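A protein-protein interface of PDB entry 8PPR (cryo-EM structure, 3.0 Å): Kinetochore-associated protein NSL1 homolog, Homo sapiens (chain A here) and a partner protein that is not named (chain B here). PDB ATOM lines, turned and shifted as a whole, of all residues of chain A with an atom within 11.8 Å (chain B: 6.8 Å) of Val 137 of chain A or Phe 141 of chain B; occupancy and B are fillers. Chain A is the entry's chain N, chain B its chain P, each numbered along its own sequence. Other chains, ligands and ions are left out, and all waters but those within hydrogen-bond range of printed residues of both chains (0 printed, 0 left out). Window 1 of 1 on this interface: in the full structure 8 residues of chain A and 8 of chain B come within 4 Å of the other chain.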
ATOM      1  N   GLN A 128      -4.409 -10.343  18.219  1.00  0.00           N
ATOM      2  CA  GLN A 128      -3.483 -10.463  19.338  1.00  0.00           C
ATOM      3  C   GLN A 128      -2.439  -9.352  19.386  1.00  0.00           C
ATOM      4  O   GLN A 128      -2.218  -8.762  20.448  1.00  0.00           O
ATOM      5  CB  GLN A 128      -2.787 -11.826  19.294  1.00  0.00           C
ATOM      6  CG  GLN A 128      -3.723 -13.009  19.480  1.00  0.00           C
ATOM      7  CD  GLN A 128      -4.385 -13.026  20.846  1.00  0.00           C
ATOM      8  OE1 GLN A 128      -3.918 -12.382  21.786  1.00  0.00           O
ATOM      9  NE2 GLN A 128      -5.481 -13.765  20.961  1.00  0.00           N
ATOM     10  N   TYR A 129      -1.783  -9.067  18.260  1.00  0.00           N
ATOM     11  CA  TYR A 129      -0.639  -8.157  18.281  1.00  0.00           C
ATOM     12  C   TYR A 129      -0.924  -6.796  18.908  1.00  0.00           C
ATOM     13  O   TYR A 129      -0.072  -6.327  19.684  1.00  0.00           O
ATOM     14  CB  TYR A 129      -0.090  -7.981  16.861  1.00  0.00           C
ATOM     15  CG  TYR A 129       0.618  -9.200  16.328  1.00  0.00           C
ATOM     16  CD1 TYR A 129       0.953 -10.255  17.167  1.00  0.00           C
ATOM     17  CD2 TYR A 129       0.976  -9.289  14.994  1.00  0.00           C
ATOM     18  CE1 TYR A 129       1.608 -11.369  16.685  1.00  0.00           C
ATOM     19  CE2 TYR A 129       1.635 -10.395  14.505  1.00  0.00           C
ATOM     20  CZ  TYR A 129       1.947 -11.433  15.351  1.00  0.00           C
ATOM     21  OH  TYR A 129       2.602 -12.538  14.860  1.00  0.00           O
ATOM     22  N   PRO A 130      -2.049  -6.121  18.640  1.00  0.00           N
ATOM     23  CA  PRO A 130      -2.242  -4.782  19.221  1.00  0.00           C
ATOM     24  C   PRO A 130      -2.131  -4.741  20.733  1.00  0.00           C
ATOM     25  O   PRO A 130      -1.649  -3.741  21.274  1.00  0.00           O
ATOM     26  CB  PRO A 130      -3.652  -4.402  18.752  1.00  0.00           C
ATOM     27  CG  PRO A 130      -3.831  -5.149  17.491  1.00  0.00           C
ATOM     28  CD  PRO A 130      -3.130  -6.456  17.695  1.00  0.00           C
ATOM     29  N   ARG A 131      -2.558  -5.791  21.434  1.00  0.00           N
ATOM     30  CA  ARG A 131      -2.451  -5.798  22.890  1.00  0.00           C
ATOM     31  C   ARG A 131      -0.994  -5.747  23.339  1.00  0.00           C
ATOM     32  O   ARG A 131      -0.621  -4.940  24.200  1.00  0.00           O
ATOM     33  CB  ARG A 131      -3.149  -7.035  23.449  1.00  0.00           C
ATOM     34  CG  ARG A 131      -3.241  -7.075  24.961  1.00  0.00           C
ATOM     35  CD  ARG A 131      -3.998  -8.312  25.401  1.00  0.00           C
ATOM     36  NE  ARG A 131      -3.257  -9.527  25.081  1.00  0.00           N
ATOM     37  CZ  ARG A 131      -3.644 -10.426  24.187  1.00  0.00           C
ATOM     38  NH1 ARG A 131      -4.763 -10.277  23.497  1.00  0.00           N
ATOM     39  NH2 ARG A 131      -2.887 -11.498  23.977  1.00  0.00           N
ATOM     40  N   LYS A 132      -0.155  -6.609  22.760  1.00  0.00           N
ATOM     41  CA  LYS A 132       1.262  -6.613  23.108  1.00  0.00           C
ATOM     42  C   LYS A 132       1.927  -5.308  22.693  1.00  0.00           C
ATOM     43  O   LYS A 132       2.781  -4.776  23.416  1.00  0.00           O
ATOM     44  CB  LYS A 132       1.958  -7.805  22.451  1.00  0.00           C
ATOM     45  CG  LYS A 132       1.423  -9.188  22.849  1.00  0.00           C
ATOM     46  CD  LYS A 132       1.761  -9.586  24.285  1.00  0.00           C
ATOM     47  CE  LYS A 132       0.646  -9.230  25.262  1.00  0.00           C
ATOM     48  NZ  LYS A 132       0.939  -9.720  26.637  1.00  0.00           N
ATOM     49  N   ILE A 133       1.547  -4.782  21.526  1.00  0.00           N
ATOM     50  CA  ILE A 133       2.049  -3.487  21.086  1.00  0.00           C
ATOM     51  C   ILE A 133       1.730  -2.417  22.117  1.00  0.00           C
ATOM     52  O   ILE A 133       2.591  -1.611  22.488  1.00  0.00           O
ATOM     53  CB  ILE A 133       1.455  -3.132  19.710  1.00  0.00           C
ATOM     54  CG1 ILE A 133       1.883  -4.152  18.651  1.00  0.00           C
ATOM     55  CG2 ILE A 133       1.824  -1.714  19.317  1.00  0.00           C
ATOM     56  CD1 ILE A 133       3.352  -4.516  18.706  1.00  0.00           C
ATOM     57  N   LEU A 134       0.492  -2.405  22.604  1.00  0.00           N
ATOM     58  CA  LEU A 134       0.077  -1.395  23.567  1.00  0.00           C
ATOM     59  C   LEU A 134       0.826  -1.555  24.882  1.00  0.00           C
ATOM     60  O   LEU A 134       1.198  -0.563  25.517  1.00  0.00           O
ATOM     61  CB  LEU A 134      -1.430  -1.487  23.782  1.00  0.00           C
ATOM     62  CG  LEU A 134      -2.096  -0.229  24.323  1.00  0.00           C
ATOM     63  CD1 LEU A 134      -1.697   0.959  23.460  1.00  0.00           C
ATOM     64  CD2 LEU A 134      -3.605  -0.402  24.346  1.00  0.00           C
ATOM     65  N   GLU A 135       1.051  -2.800  25.308  1.00  0.00           N
ATOM     66  CA  GLU A 135       1.814  -3.031  26.531  1.00  0.00           C
ATOM     67  C   GLU A 135       3.242  -2.513  26.402  1.00  0.00           C
ATOM     68  O   GLU A 135       3.760  -1.853  27.314  1.00  0.00           O
ATOM     69  CB  GLU A 135       1.815  -4.520  26.873  1.00  0.00           C
ATOM     70  CG  GLU A 135       2.730  -4.886  28.025  1.00  0.00           C
ATOM     71  CD  GLU A 135       2.272  -6.129  28.757  1.00  0.00           C
ATOM     72  OE1 GLU A 135       1.291  -6.757  28.307  1.00  0.00           O
ATOM     73  OE2 GLU A 135       2.889  -6.474  29.786  1.00  0.00           O
ATOM     74  N   CYS A 136       3.892  -2.799  25.271  1.00  0.00           N
ATOM     75  CA  CYS A 136       5.244  -2.295  25.049  1.00  0.00           C
ATOM     76  C   CYS A 136       5.260  -0.773  25.005  1.00  0.00           C
ATOM     77  O   CYS A 136       6.187  -0.138  25.522  1.00  0.00           O
ATOM     78  CB  CYS A 136       5.818  -2.876  23.756  1.00  0.00           C
ATOM     79  SG  CYS A 136       5.910  -4.679  23.721  1.00  0.00           S
ATOM     80  N   VAL A 137       4.241  -0.175  24.387  1.00  0.00           N
ATOM     81  CA  VAL A 137       4.154   1.280  24.325  1.00  0.00           C
ATOM     82  C   VAL A 137       4.009   1.865  25.724  1.00  0.00           C
ATOM     83  O   VAL A 137       4.641   2.874  26.057  1.00  0.00           O
ATOM     84  CB  VAL A 137       2.991   1.703  23.408  1.00  0.00           C
ATOM     85  CG1 VAL A 137       2.662   3.173  23.603  1.00  0.00           C
ATOM     86  CG2 VAL A 137       3.340   1.424  21.955  1.00  0.00           C
ATOM     87  N   ILE A 138       3.178   1.244  26.561  1.00  0.00           N
ATOM     88  CA  ILE A 138       3.011   1.706  27.937  1.00  0.00           C
ATOM     89  C   ILE A 138       4.331   1.625  28.690  1.00  0.00           C
ATOM     90  O   ILE A 138       4.714   2.555  29.413  1.00  0.00           O
ATOM     91  CB  ILE A 138       1.910   0.899  28.647  1.00  0.00           C
ATOM     92  CG1 ILE A 138       0.541   1.283  28.096  1.00  0.00           C
ATOM     93  CG2 ILE A 138       1.964   1.122  30.149  1.00  0.00           C
ATOM     94  CD1 ILE A 138       0.246   2.751  28.269  1.00  0.00           C
ATOM     95  N   LYS A 139       5.040   0.506  28.541  1.00  0.00           N
ATOM     96  CA  LYS A 139       6.316   0.356  29.233  1.00  0.00           C
ATOM     97  C   LYS A 139       7.310   1.422  28.789  1.00  0.00           C
ATOM     98  O   LYS A 139       7.978   2.049  29.624  1.00  0.00           O
ATOM     99  CB  LYS A 139       6.880  -1.043  28.989  1.00  0.00           C
ATOM    100  CG  LYS A 139       6.281  -2.109  29.890  1.00  0.00           C
ATOM    101  CD  LYS A 139       7.082  -3.397  29.836  1.00  0.00           C
ATOM    102  CE  LYS A 139       6.297  -4.555  30.428  1.00  0.00           C
ATOM    103  NZ  LYS A 139       6.031  -4.360  31.880  1.00  0.00           N
ATOM    104  N   THR A 140       7.404   1.657  27.478  1.00  0.00           N
ATOM    105  CA  THR A 140       8.323   2.669  26.970  1.00  0.00           C
ATOM    106  C   THR A 140       7.937   4.059  27.458  1.00  0.00           C
ATOM    107  O   THR A 140       8.805   4.859  27.827  1.00  0.00           O
ATOM    108  CB  THR A 140       8.356   2.624  25.442  1.00  0.00           C
ATOM    109  OG1 THR A 140       8.734   1.311  25.010  1.00  0.00           O
ATOM    110  CG2 THR A 140       9.358   3.630  24.903  1.00  0.00           C
ATOM    111  N   ILE A 141       6.638   4.363  27.471  1.00  0.00           N
ATOM    112  CA  ILE A 141       6.174   5.677  27.909  1.00  0.00           C
ATOM    113  C   ILE A 141       6.518   5.899  29.375  1.00  0.00           C
ATOM    114  O   ILE A 141       7.003   6.967  29.764  1.00  0.00           O
ATOM    115  CB  ILE A 141       4.662   5.818  27.661  1.00  0.00           C
ATOM    116  CG1 ILE A 141       4.387   6.126  26.188  1.00  0.00           C
ATOM    117  CG2 ILE A 141       4.065   6.896  28.554  1.00  0.00           C
ATOM    118  CD1 ILE A 141       2.915   6.249  25.859  1.00  0.00           C
ATOM    119  N   LYS A 142       6.267   4.890  30.212  1.00  0.00           N
ATOM    120  CA  LYS A 142       6.568   5.024  31.632  1.00  0.00           C
ATOM    121  C   LYS A 142       8.065   5.178  31.864  1.00  0.00           C
ATOM    122  O   LYS A 142       8.494   5.987  32.696  1.00  0.00           O
ATOM    123  CB  LYS A 142       6.021   3.820  32.397  1.00  0.00           C
ATOM    124  CG  LYS A 142       4.506   3.757  32.428  1.00  0.00           C
ATOM    125  CD  LYS A 142       4.022   2.462  33.051  1.00  0.00           C
ATOM    126  CE  LYS A 142       4.386   2.401  34.524  1.00  0.00           C
ATOM    127  NZ  LYS A 142       3.636   3.410  35.319  1.00  0.00           N
ATOM    128  N   ALA A 143       8.878   4.411  31.131  1.00  0.00           N
ATOM    129  CA  ALA A 143      10.324   4.545  31.264  1.00  0.00           C
ATOM    130  C   ALA A 143      10.787   5.935  30.847  1.00  0.00           C
ATOM    131  O   ALA A 143      11.657   6.529  31.497  1.00  0.00           O
ATOM    132  CB  ALA A 143      11.027   3.470  30.437  1.00  0.00           C
ATOM    133  N   LYS A 144      10.222   6.468  29.764  1.00  0.00           N
ATOM    134  CA  LYS A 144      10.589   7.807  29.319  1.00  0.00           C
ATOM    135  C   LYS A 144      10.186   8.857  30.346  1.00  0.00           C
ATOM    136  O   LYS A 144      10.939   9.801  30.609  1.00  0.00           O
ATOM    137  CB  LYS A 144       9.948   8.099  27.964  1.00  0.00           C
ATOM    138  CG  LYS A 144      10.622   7.380  26.814  1.00  0.00           C
ATOM    139  CD  LYS A 144       9.986   7.738  25.485  1.00  0.00           C
ATOM    140  CE  LYS A 144      10.679   7.018  24.342  1.00  0.00           C
ATOM    141  NZ  LYS A 144      12.067   7.516  24.138  1.00  0.00           N
ATOM    142  N   GLN A 145       9.001   8.706  30.938  1.00  0.00           N
ATOM    143  CA  GLN A 145       8.581   9.627  31.989  1.00  0.00           C
ATOM    144  C   GLN A 145       9.543   9.581  33.167  1.00  0.00           C
ATOM    145  O   GLN A 145       9.933  10.624  33.706  1.00  0.00           O
ATOM    146  CB  GLN A 145       7.161   9.290  32.445  1.00  0.00           C
ATOM    147  CG  GLN A 145       6.076   9.529  31.402  1.00  0.00           C
ATOM    148  CD  GLN A 145       5.722  10.997  31.223  1.00  0.00           C
ATOM    149  OE1 GLN A 145       6.589  11.870  31.241  1.00  0.00           O
ATOM    150  NE2 GLN A 145       4.435  11.271  31.048  1.00  0.00           N
ATOM    151  N   GLU A 146       9.947   8.375  33.572  1.00  0.00           N
ATOM    152  CA  GLU A 146      10.860   8.246  34.702  1.00  0.00           C
ATOM    153  C   GLU A 146      12.218   8.868  34.399  1.00  0.00           C
ATOM    154  O   GLU A 146      12.782   9.580  35.237  1.00  0.00           O
ATOM    155  CB  GLU A 146      11.015   6.775  35.083  1.00  0.00           C
ATOM    156  CG  GLU A 146      11.757   6.554  36.390  1.00  0.00           C
ATOM    157  CD  GLU A 146      11.875   5.088  36.751  1.00  0.00           C
ATOM    158  OE1 GLU A 146      11.989   4.254  35.828  1.00  0.00           O
ATOM    159  OE2 GLU A 146      11.855   4.768  37.958  1.00  0.00           O
ATOM    160  N   LEU A 148      12.873  11.216  32.256  1.00  0.00           N
ATOM    161  CA  LEU A 148      12.725  12.665  32.202  1.00  0.00           C
ATOM    162  C   LEU A 148      12.622  13.263  33.596  1.00  0.00           C
ATOM    163  O   LEU A 148      13.132  14.362  33.838  1.00  0.00           O
ATOM    164  CB  LEU A 148      11.501  13.040  31.369  1.00  0.00           C
ATOM    165  CG  LEU A 148      11.547  14.418  30.707  1.00  0.00           C
ATOM    166  CD1 LEU A 148      12.918  14.678  30.101  1.00  0.00           C
ATOM    167  CD2 LEU A 148      10.462  14.541  29.651  1.00  0.00           C
ATOM    168  N   MET B 137      -2.908   3.241  19.553  1.00  0.00           N
ATOM    169  CA  MET B 137      -1.859   3.867  20.348  1.00  0.00           C
ATOM    170  C   MET B 137      -1.934   5.390  20.385  1.00  0.00           C
ATOM    171  O   MET B 137      -1.104   6.012  21.056  1.00  0.00           O
ATOM    172  CB  MET B 137      -0.483   3.404  19.850  1.00  0.00           C
ATOM    173  CG  MET B 137      -0.106   3.828  18.443  1.00  0.00           C
ATOM    174  SD  MET B 137       1.507   3.157  17.989  1.00  0.00           S
ATOM    175  CE  MET B 137       1.697   3.766  16.317  1.00  0.00           C
ATOM    176  N   ALA B 138      -2.897   6.007  19.701  1.00  0.00           N
ATOM    177  CA  ALA B 138      -3.058   7.456  19.815  1.00  0.00           C
ATOM    178  C   ALA B 138      -3.422   7.929  21.220  1.00  0.00           C
ATOM    179  O   ALA B 138      -2.767   8.864  21.716  1.00  0.00           O
ATOM    180  CB  ALA B 138      -4.087   7.932  18.785  1.00  0.00           C
ATOM    181  N   PRO B 139      -4.435   7.369  21.904  1.00  0.00           N
ATOM    182  CA  PRO B 139      -4.876   7.987  23.171  1.00  0.00           C
ATOM    183  C   PRO B 139      -3.797   8.062  24.236  1.00  0.00           C
ATOM    184  O   PRO B 139      -3.738   9.043  24.989  1.00  0.00           O
ATOM    185  CB  PRO B 139      -6.034   7.079  23.611  1.00  0.00           C
ATOM    186  CG  PRO B 139      -6.519   6.449  22.360  1.00  0.00           C
ATOM    187  CD  PRO B 139      -5.284   6.215  21.551  1.00  0.00           C
ATOM    188  N   TYR B 140      -2.939   7.050  24.325  1.00  0.00           N
ATOM    189  CA  TYR B 140      -1.920   7.051  25.369  1.00  0.00           C
ATOM    190  C   TYR B 140      -0.842   8.085  25.076  1.00  0.00           C
ATOM    191  O   TYR B 140      -0.330   8.739  25.995  1.00  0.00           O
ATOM    192  CB  TYR B 140      -1.328   5.652  25.505  1.00  0.00           C
ATOM    193  CG  TYR B 140      -2.317   4.653  26.057  1.00  0.00           C
ATOM    194  CD1 TYR B 140      -3.493   5.074  26.665  1.00  0.00           C
ATOM    195  CD2 TYR B 140      -2.091   3.293  25.949  1.00  0.00           C
ATOM    196  CE1 TYR B 140      -4.403   4.166  27.166  1.00  0.00           C
ATOM    197  CE2 TYR B 140      -2.991   2.377  26.450  1.00  0.00           C
ATOM    198  CZ  TYR B 140      -4.147   2.817  27.053  1.00  0.00           C
ATOM    199  OH  TYR B 140      -5.048   1.903  27.547  1.00  0.00           O
ATOM    200  N   PHE B 141      -0.496   8.257  23.800  1.00  0.00           N
ATOM    201  CA  PHE B 141       0.399   9.343  23.423  1.00  0.00           C
ATOM    202  C   PHE B 141      -0.225  10.694  23.739  1.00  0.00           C
ATOM    203  O   PHE B 141       0.468  11.620  24.177  1.00  0.00           O
ATOM    204  CB  PHE B 141       0.748   9.246  21.940  1.00  0.00           C
ATOM    205  CG  PHE B 141       1.899   8.332  21.649  1.00  0.00           C
ATOM    206  CD1 PHE B 141       1.735   6.959  21.680  1.00  0.00           C
ATOM    207  CD2 PHE B 141       3.148   8.846  21.351  1.00  0.00           C
ATOM    208  CE1 PHE B 141       2.793   6.115  21.413  1.00  0.00           C
ATOM    209  CE2 PHE B 141       4.211   8.008  21.086  1.00  0.00           C
ATOM    210  CZ  PHE B 141       4.033   6.640  21.115  1.00  0.00           C
ATOM    211  N   LEU B 142      -1.537  10.825  23.525  1.00  0.00           N
ATOM    212  CA  LEU B 142      -2.220  12.063  23.888  1.00  0.00           C
ATOM    213  C   LEU B 142      -2.127  12.323  25.385  1.00  0.00           C
ATOM    214  O   LEU B 142      -1.875  13.455  25.816  1.00  0.00           O
ATOM    215  CB  LEU B 142      -3.682  11.998  23.448  1.00  0.00           C
ATOM    216  CG  LEU B 142      -3.960  12.173  21.956  1.00  0.00           C
ATOM    217  CD1 LEU B 142      -5.428  12.488  21.724  1.00  0.00           C
ATOM    218  CD2 LEU B 142      -3.082  13.266  21.374  1.00  0.00           C
ATOM    219  N   GLN B 143      -2.329  11.281  26.192  1.00  0.00           N
ATOM    220  CA  GLN B 143      -2.222  11.424  27.642  1.00  0.00           C
ATOM    221  C   GLN B 143      -0.815  11.834  28.057  1.00  0.00           C
ATOM    222  O   GLN B 143      -0.638  12.709  28.918  1.00  0.00           O
ATOM    223  CB  GLN B 143      -2.617  10.112  28.316  1.00  0.00           C
ATOM    224  CG  GLN B 143      -2.272  10.038  29.790  1.00  0.00           C
ATOM    225  CD  GLN B 143      -2.074   8.613  30.264  1.00  0.00           C
ATOM    226  OE1 GLN B 143      -0.959   8.204  30.587  1.00  0.00           O
ATOM    227  NE2 GLN B 143      -3.157   7.846  30.302  1.00  0.00           N
ATOM    228  N   GLN B 144       0.200  11.207  27.459  1.00  0.00           N
ATOM    229  CA  GLN B 144       1.581  11.565  27.765  1.00  0.00           C
ATOM    230  C   GLN B 144       1.867  13.013  27.390  1.00  0.00           C
ATOM    231  O   GLN B 144       2.526  13.741  28.143  1.00  0.00           O
ATOM    232  CB  GLN B 144       2.537  10.626  27.033  1.00  0.00           C
ATOM    233  CG  GLN B 144       3.994  10.809  27.409  1.00  0.00           C
ATOM    234  CD  GLN B 144       4.930  10.494  26.261  1.00  0.00           C
ATOM    235  OE1 GLN B 144       4.501  10.360  25.115  1.00  0.00           O
ATOM    236  NE2 GLN B 144       6.217  10.376  26.562  1.00  0.00           N
ATOM    237  N   ARG B 145       1.382  13.442  26.224  1.00  0.00           N
ATOM    238  CA  ARG B 145       1.557  14.827  25.806  1.00  0.00           C
ATOM    239  C   ARG B 145       0.897  15.783  26.788  1.00  0.00           C
ATOM    240  O   ARG B 145       1.465  16.827  27.125  1.00  0.00           O
ATOM    241  CB  ARG B 145       0.981  15.023  24.407  1.00  0.00           C
ATOM    242  CG  ARG B 145       0.992  16.461  23.933  1.00  0.00           C
ATOM    243  CD  ARG B 145       0.100  16.624  22.721  1.00  0.00           C
ATOM    244  NE  ARG B 145      -1.305  16.454  23.069  1.00  0.00           N
ATOM    245  CZ  ARG B 145      -2.314  16.654  22.234  1.00  0.00           C
ATOM    246  NH1 ARG B 145      -2.110  17.035  20.983  1.00  0.00           N
ATOM    247  NH2 ARG B 145      -3.558  16.468  22.663  1.00  0.00           N
ATOM    248  N   ASP B 146      -0.308  15.445  27.250  1.00  0.00           N
ATOM    249  CA  ASP B 146      -0.997  16.303  28.210  1.00  0.00           C
ATOM    250  C   ASP B 146      -0.214  16.411  29.512  1.00  0.00           C
ATOM    251  O   ASP B 146      -0.062  17.507  30.067  1.00  0.00           O
ATOM    252  CB  ASP B 146      -2.401  15.765  28.470  1.00  0.00           C
ATOM    253  CG  ASP B 146      -3.258  15.754  27.222  1.00  0.00           C
ATOM    254  OD1 ASP B 146      -2.868  16.402  26.229  1.00  0.00           O
ATOM    255  OD2 ASP B 146      -4.316  15.092  27.232  1.00  0.00           O
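Val 137 of chain A touches just one residue of chain B: Phe 141.
Phe 141 of chain B touches just one residue of chain A: Val 137 (3.7 Å).
No residue of chain A comes within 4 Å of Met 137 of chain B.
No residue of chain A comes within 4 Å of Pro 139 of chain B.
Gln 144 of chain B touches just one residue of chain A: Gln 145.
No residue of chain A comes within 4 Å of Arg 145 of chain B.
Printed residues of chain B within 4 Å of Ile 138 of chain A: Tyr 140 (3.3 Å).
Of the printed residues of chain B, Gln 145 of chain A touches Gln 144.
Of the printed residues of chain B, Leu 134 of chain A touches Tyr 140 (3.4 Å).
Of the printed residues of chain A, Tyr 140 of chain B touches Leu 134 (3.4 Å) and Ile 138 (3.3 Å).
Tyr 129 of chain A touches none of the printed residues of chain B.
Among the printed residues, pairs that only touch across the chains: Ile 138 of chain A with Tyr 140 of chain B (3.3 Å), Leu 134 of chain A with Tyr 140 of chain B (3.4 Å), Val 137 of chain A with Phe 141 of chain B (3.7 Å) and Gln 145 of chain A with Gln 144 of chain B (3.7 Å).
Of the 10 printed residues of chain B, 3 touch a printed residue of chain A.
Printed residues of chain B that touch a printed residue of chain A: Tyr 140, Phe 141 and Gln 144.
Along chain B the printed residues that touch a printed residue of chain A span positions 140 to 144.
Hydrophobic or aromatic side chains of chain A that line the printed part of chain B: Leu 134, Val 137 and Ile 138.
Among the printed residues, 4 pairs touch across the chains.
Among the printed residues, no Asp or Glu carboxylate lies within 4 Å of a Lys or Arg side-chain nitrogen of the other chain.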
